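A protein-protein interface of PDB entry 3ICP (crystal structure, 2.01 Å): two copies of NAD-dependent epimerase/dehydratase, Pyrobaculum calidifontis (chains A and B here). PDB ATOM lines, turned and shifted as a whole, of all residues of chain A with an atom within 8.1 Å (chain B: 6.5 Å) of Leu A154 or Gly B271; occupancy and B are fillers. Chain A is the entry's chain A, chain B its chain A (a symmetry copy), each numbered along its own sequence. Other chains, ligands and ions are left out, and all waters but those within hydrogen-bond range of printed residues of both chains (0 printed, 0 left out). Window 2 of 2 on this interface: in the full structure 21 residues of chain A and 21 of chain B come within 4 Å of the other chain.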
ATOM      1  N   ARG A 101       7.223 -24.951  15.161  1.00  0.00           N
ATOM      2  CA  ARG A 101       6.380 -23.771  15.067  1.00  0.00           C
ATOM      3  C   ARG A 101       6.863 -22.668  16.003  1.00  0.00           C
ATOM      4  O   ARG A 101       7.026 -21.526  15.587  1.00  0.00           O
ATOM      5  CB  ARG A 101       4.930 -24.127  15.419  1.00  0.00           C
ATOM      6  CG  ARG A 101       3.995 -22.918  15.479  1.00  0.00           C
ATOM      7  CD  ARG A 101       2.577 -23.310  15.901  1.00  0.00           C
ATOM      8  NE  ARG A 101       2.468 -23.642  17.321  1.00  0.00           N
ATOM      9  CZ  ARG A 101       2.394 -22.746  18.302  1.00  0.00           C
ATOM     10  NH1 ARG A 101       2.417 -21.450  18.020  1.00  0.00           N
ATOM     11  NH2 ARG A 101       2.294 -23.142  19.564  1.00  0.00           N
ATOM     12  N   MET A 147      -0.728 -34.329  10.443  1.00  0.00           N
ATOM     13  CA  MET A 147      -0.353 -33.219  11.311  1.00  0.00           C
ATOM     14  C   MET A 147       0.695 -32.324  10.647  1.00  0.00           C
ATOM     15  O   MET A 147       0.600 -31.097  10.725  1.00  0.00           O
ATOM     16  CB  MET A 147       0.183 -33.740  12.647  1.00  0.00           C
ATOM     17  CG  MET A 147      -0.855 -34.478  13.472  1.00  0.00           C
ATOM     18  SD  MET A 147      -0.309 -34.793  15.156  1.00  0.00           S
ATOM     19  CE  MET A 147       0.934 -36.098  14.861  1.00  0.00           C
ATOM     20  N   CYS A 148       1.691 -32.934  10.002  1.00  0.00           N
ATOM     21  CA  CYS A 148       2.744 -32.179   9.310  1.00  0.00           C
ATOM     22  C   CYS A 148       2.173 -31.301   8.206  1.00  0.00           C
ATOM     23  O   CYS A 148       2.575 -30.149   8.045  1.00  0.00           O
ATOM     24  CB  CYS A 148       3.771 -33.112   8.658  1.00  0.00           C
ATOM     25  SG  CYS A 148       4.950 -33.891   9.778  1.00  0.00           S
ATOM     26  N   ALA A 149       1.264 -31.871   7.420  1.00  0.00           N
ATOM     27  CA  ALA A 149       0.651 -31.152   6.308  1.00  0.00           C
ATOM     28  C   ALA A 149      -0.166 -29.981   6.828  1.00  0.00           C
ATOM     29  O   ALA A 149      -0.184 -28.909   6.228  1.00  0.00           O
ATOM     30  CB  ALA A 149      -0.236 -32.097   5.488  1.00  0.00           C
ATOM     31  N   THR A 150      -0.832 -30.186   7.958  1.00  0.00           N
ATOM     32  CA  THR A 150      -1.649 -29.136   8.555  1.00  0.00           C
ATOM     33  C   THR A 150      -0.776 -27.992   9.074  1.00  0.00           C
ATOM     34  O   THR A 150      -1.105 -26.818   8.885  1.00  0.00           O
ATOM     35  CB  THR A 150      -2.516 -29.706   9.704  1.00  0.00           C
ATOM     36  OG1 THR A 150      -3.382 -30.724   9.183  1.00  0.00           O
ATOM     37  CG2 THR A 150      -3.361 -28.615  10.329  1.00  0.00           C
ATOM     38  N   TYR A 151       0.335 -28.330   9.728  1.00  0.00           N
ATOM     39  CA  TYR A 151       1.239 -27.310  10.255  1.00  0.00           C
ATOM     40  C   TYR A 151       1.841 -26.497   9.106  1.00  0.00           C
ATOM     41  O   TYR A 151       2.174 -25.320   9.275  1.00  0.00           O
ATOM     42  CB  TYR A 151       2.349 -27.956  11.106  1.00  0.00           C
ATOM     43  CG  TYR A 151       2.007 -28.042  12.585  1.00  0.00           C
ATOM     44  CD1 TYR A 151       0.912 -28.791  13.033  1.00  0.00           C
ATOM     45  CD2 TYR A 151       2.718 -27.296  13.530  1.00  0.00           C
ATOM     46  CE1 TYR A 151       0.527 -28.778  14.381  1.00  0.00           C
ATOM     47  CE2 TYR A 151       2.336 -27.284  14.883  1.00  0.00           C
ATOM     48  CZ  TYR A 151       1.237 -28.020  15.295  1.00  0.00           C
ATOM     49  OH  TYR A 151       0.814 -27.955  16.609  1.00  0.00           O
ATOM     50  N   ALA A 152       1.969 -27.127   7.941  1.00  0.00           N
ATOM     51  CA  ALA A 152       2.511 -26.458   6.763  1.00  0.00           C
ATOM     52  C   ALA A 152       1.495 -25.456   6.229  1.00  0.00           C
ATOM     53  O   ALA A 152       1.838 -24.316   5.920  1.00  0.00           O
ATOM     54  CB  ALA A 152       2.849 -27.482   5.679  1.00  0.00           C
ATOM     55  N   ARG A 153       0.241 -25.882   6.129  1.00  0.00           N
ATOM     56  CA  ARG A 153      -0.811 -25.011   5.621  1.00  0.00           C
ATOM     57  C   ARG A 153      -1.208 -23.914   6.600  1.00  0.00           C
ATOM     58  O   ARG A 153      -1.482 -22.781   6.197  1.00  0.00           O
ATOM     59  CB  ARG A 153      -2.056 -25.831   5.265  1.00  0.00           C
ATOM     60  CG  ARG A 153      -1.886 -26.748   4.061  1.00  0.00           C
ATOM     61  CD  ARG A 153      -3.211 -27.405   3.689  1.00  0.00           C
ATOM     62  NE  ARG A 153      -3.653 -28.348   4.710  1.00  0.00           N
ATOM     63  CZ  ARG A 153      -3.441 -29.660   4.663  1.00  0.00           C
ATOM     64  NH1 ARG A 153      -2.801 -30.197   3.633  1.00  0.00           N
ATOM     65  NH2 ARG A 153      -3.847 -30.434   5.661  1.00  0.00           N
ATOM     66  N   LEU A 154      -1.226 -24.250   7.888  1.00  0.00           N
ATOM     67  CA  LEU A 154      -1.634 -23.305   8.925  1.00  0.00           C
ATOM     68  C   LEU A 154      -0.551 -22.390   9.496  1.00  0.00           C
ATOM     69  O   LEU A 154      -0.764 -21.183   9.631  1.00  0.00           O
ATOM     70  CB  LEU A 154      -2.288 -24.071  10.082  1.00  0.00           C
ATOM     71  CG  LEU A 154      -2.757 -23.262  11.298  1.00  0.00           C
ATOM     72  CD1 LEU A 154      -3.819 -22.244  10.880  1.00  0.00           C
ATOM     73  CD2 LEU A 154      -3.306 -24.211  12.360  1.00  0.00           C
ATOM     74  N   PHE A 155       0.602 -22.960   9.832  1.00  0.00           N
ATOM     75  CA  PHE A 155       1.674 -22.178  10.434  1.00  0.00           C
ATOM     76  C   PHE A 155       2.843 -21.856   9.505  1.00  0.00           C
ATOM     77  O   PHE A 155       3.791 -21.185   9.911  1.00  0.00           O
ATOM     78  CB  PHE A 155       2.184 -22.911  11.677  1.00  0.00           C
ATOM     79  CG  PHE A 155       1.127 -23.126  12.733  1.00  0.00           C
ATOM     80  CD1 PHE A 155       0.527 -22.036  13.362  1.00  0.00           C
ATOM     81  CD2 PHE A 155       0.746 -24.412  13.111  1.00  0.00           C
ATOM     82  CE1 PHE A 155      -0.438 -22.223  14.353  1.00  0.00           C
ATOM     83  CE2 PHE A 155      -0.221 -24.611  14.104  1.00  0.00           C
ATOM     84  CZ  PHE A 155      -0.812 -23.516  14.725  1.00  0.00           C
ATOM     85  N   GLY A 156       2.779 -22.328   8.264  1.00  0.00           N
ATOM     86  CA  GLY A 156       3.857 -22.058   7.331  1.00  0.00           C
ATOM     87  C   GLY A 156       5.087 -22.940   7.506  1.00  0.00           C
ATOM     88  O   GLY A 156       6.113 -22.709   6.864  1.00  0.00           O
ATOM     89  N   VAL A 157       5.000 -23.940   8.379  1.00  0.00           N
ATOM     90  CA  VAL A 157       6.113 -24.862   8.588  1.00  0.00           C
ATOM     91  C   VAL A 157       6.036 -25.885   7.462  1.00  0.00           C
ATOM     92  O   VAL A 157       5.347 -26.905   7.585  1.00  0.00           O
ATOM     93  CB  VAL A 157       5.984 -25.591   9.944  1.00  0.00           C
ATOM     94  CG1 VAL A 157       7.178 -26.522  10.156  1.00  0.00           C
ATOM     95  CG2 VAL A 157       5.886 -24.572  11.059  1.00  0.00           C
ATOM     96  N   PRO A 226       3.324 -25.914   0.268  1.00  0.00           N
ATOM     97  CA  PRO A 226       3.476 -26.077   1.716  1.00  0.00           C
ATOM     98  C   PRO A 226       3.852 -27.512   2.116  1.00  0.00           C
ATOM     99  O   PRO A 226       4.727 -27.724   2.959  1.00  0.00           O
ATOM    100  CB  PRO A 226       2.100 -25.682   2.249  1.00  0.00           C
ATOM    101  CG  PRO A 226       1.626 -24.676   1.240  1.00  0.00           C
ATOM    102  CD  PRO A 226       2.004 -25.337  -0.058  1.00  0.00           C
ATOM    103  N   LEU B  77     -11.024 -22.328  17.653  1.00  0.00           N
ATOM    104  CA  LEU B  77      -9.884 -23.219  17.470  1.00  0.00           C
ATOM    105  C   LEU B  77      -8.521 -22.525  17.524  1.00  0.00           C
ATOM    106  O   LEU B  77      -7.530 -23.127  17.946  1.00  0.00           O
ATOM    107  CB  LEU B  77     -10.025 -23.973  16.140  1.00  0.00           C
ATOM    108  CG  LEU B  77     -11.340 -24.736  15.930  1.00  0.00           C
ATOM    109  CD1 LEU B  77     -11.312 -25.466  14.588  1.00  0.00           C
ATOM    110  CD2 LEU B  77     -11.556 -25.716  17.078  1.00  0.00           C
ATOM    111  N   SER B  78      -8.466 -21.264  17.106  1.00  0.00           N
ATOM    112  CA  SER B  78      -7.209 -20.526  17.104  1.00  0.00           C
ATOM    113  C   SER B  78      -6.836 -19.918  18.455  1.00  0.00           C
ATOM    114  O   SER B  78      -5.735 -19.390  18.608  1.00  0.00           O
ATOM    115  CB  SER B  78      -7.241 -19.419  16.046  1.00  0.00           C
ATOM    116  OG  SER B  78      -8.159 -18.393  16.388  1.00  0.00           O
ATOM    117  N   PRO B 133      -7.268 -30.606   6.438  1.00  0.00           N
ATOM    118  CA  PRO B 133      -7.570 -29.726   7.567  1.00  0.00           C
ATOM    119  C   PRO B 133      -6.638 -28.522   7.649  1.00  0.00           C
ATOM    120  O   PRO B 133      -5.448 -28.622   7.334  1.00  0.00           O
ATOM    121  CB  PRO B 133      -7.439 -30.655   8.774  1.00  0.00           C
ATOM    122  CG  PRO B 133      -6.357 -31.606   8.346  1.00  0.00           C
ATOM    123  CD  PRO B 133      -6.710 -31.893   6.898  1.00  0.00           C
ATOM    124  N   ILE B 134      -7.191 -27.386   8.063  1.00  0.00           N
ATOM    125  CA  ILE B 134      -6.430 -26.146   8.193  1.00  0.00           C
ATOM    126  C   ILE B 134      -6.317 -25.729   9.659  1.00  0.00           C
ATOM    127  O   ILE B 134      -5.779 -24.666   9.974  1.00  0.00           O
ATOM    128  CB  ILE B 134      -7.076 -24.995   7.385  1.00  0.00           C
ATOM    129  CG1 ILE B 134      -8.533 -24.814   7.804  1.00  0.00           C
ATOM    130  CG2 ILE B 134      -6.963 -25.290   5.888  1.00  0.00           C
ATOM    131  CD1 ILE B 134      -9.172 -23.540   7.270  1.00  0.00           C
ATOM    132  N   SER B 135      -6.846 -26.560  10.554  1.00  0.00           N
ATOM    133  CA  SER B 135      -6.747 -26.278  11.979  1.00  0.00           C
ATOM    134  C   SER B 135      -6.188 -27.512  12.680  1.00  0.00           C
ATOM    135  O   SER B 135      -6.282 -28.628  12.161  1.00  0.00           O
ATOM    136  CB  SER B 135      -8.116 -25.917  12.570  1.00  0.00           C
ATOM    137  OG  SER B 135      -8.974 -27.053  12.611  1.00  0.00           O
ATOM    138  N   VAL B 136      -5.585 -27.309  13.846  1.00  0.00           N
ATOM    139  CA  VAL B 136      -5.027 -28.421  14.606  1.00  0.00           C
ATOM    140  C   VAL B 136      -6.168 -29.365  14.981  1.00  0.00           C
ATOM    141  O   VAL B 136      -6.023 -30.587  14.956  1.00  0.00           O
ATOM    142  CB  VAL B 136      -4.314 -27.917  15.890  1.00  0.00           C
ATOM    143  CG1 VAL B 136      -3.760 -29.096  16.687  1.00  0.00           C
ATOM    144  CG2 VAL B 136      -3.189 -26.959  15.509  1.00  0.00           C
ATOM    145  N   GLY B 271      -7.326 -20.540  11.251  1.00  0.00           N
ATOM    146  CA  GLY B 271      -7.627 -21.887  10.796  1.00  0.00           C
ATOM    147  C   GLY B 271      -9.111 -22.204  10.751  1.00  0.00           C
ATOM    148  O   GLY B 271      -9.512 -23.364  10.846  1.00  0.00           O
ATOM    149  N   ASP B 272      -9.935 -21.172  10.605  1.00  0.00           N
ATOM    150  CA  ASP B 272     -11.380 -21.365  10.547  1.00  0.00           C
ATOM    151  C   ASP B 272     -11.862 -21.516   9.106  1.00  0.00           C
ATOM    152  O   ASP B 272     -11.595 -20.655   8.262  1.00  0.00           O
ATOM    153  CB  ASP B 272     -12.102 -20.185  11.207  1.00  0.00           C
ATOM    154  CG  ASP B 272     -13.622 -20.295  11.121  1.00  0.00           C
ATOM    155  OD1 ASP B 272     -14.182 -21.327  11.555  1.00  0.00           O
ATOM    156  OD2 ASP B 272     -14.263 -19.344  10.624  1.00  0.00           O
ATOM    157  N   VAL B 273     -12.557 -22.615   8.824  1.00  0.00           N
ATOM    158  CA  VAL B 273     -13.095 -22.848   7.486  1.00  0.00           C
ATOM    159  C   VAL B 273     -14.155 -21.781   7.239  1.00  0.00           C
ATOM    160  O   VAL B 273     -15.022 -21.549   8.081  1.00  0.00           O
ATOM    161  CB  VAL B 273     -13.734 -24.244   7.374  1.00  0.00           C
ATOM    162  CG1 VAL B 273     -14.379 -24.419   5.997  1.00  0.00           C
ATOM    163  CG2 VAL B 273     -12.678 -25.315   7.612  1.00  0.00           C
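No position is printed for both chains.
Hydrophobic or aromatic side chains of chain B within 4 Å of the printed part of chain A: Pro B133.
Printed residues of chain A that touch a printed residue of chain B: Thr A150, Arg A153 and Leu A154.
Hydrophobic or aromatic side chains of chain A within 4 Å of the printed part of chain B: Leu A154.
Among the printed residues, 5 pairs touch across the chains.
Among the printed residues, no Asp or Glu carboxylate lies within 4 Å of a Lys or Arg side-chain nitrogen of the other chain.
The side-chain hydroxyl (OG1) of Thr A150 sits close to the backbone carbonyl oxygen (O) of Pro B133, 3.5 Å away.
O of Pro B133 lies within hydrogen-bond range of NH2 of Arg A153 (2.9 Å).
Among the printed residues, pairs that only touch across the chains: Thr A150 with Ser B135, Leu A154 with Ile B134 and Leu A154 with Gly B271.
Of the printed residues of chain B, Arg A153 touches Pro B133 (2.9 Å).
Leu A154 touches two residues of chain B.
Of the printed residues of chain A, Pro B133 touches Thr A150 and Arg A153.
Printed residues of chain A within 4 Å of Ile B134: Leu A154 (3.2 Å).
Of chain A, only Leu A154 (3.8 Å) comes within 4 Å of Gly B271.
Val B273 touches none of the printed residues of chain A.
The nearest residue of chain B that does not touch Leu A154 is Ser B135 (4.03 Å).
The nearest printed residue of chain A that does not touch Gly B271 is Arg A153 (7.7 Å).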
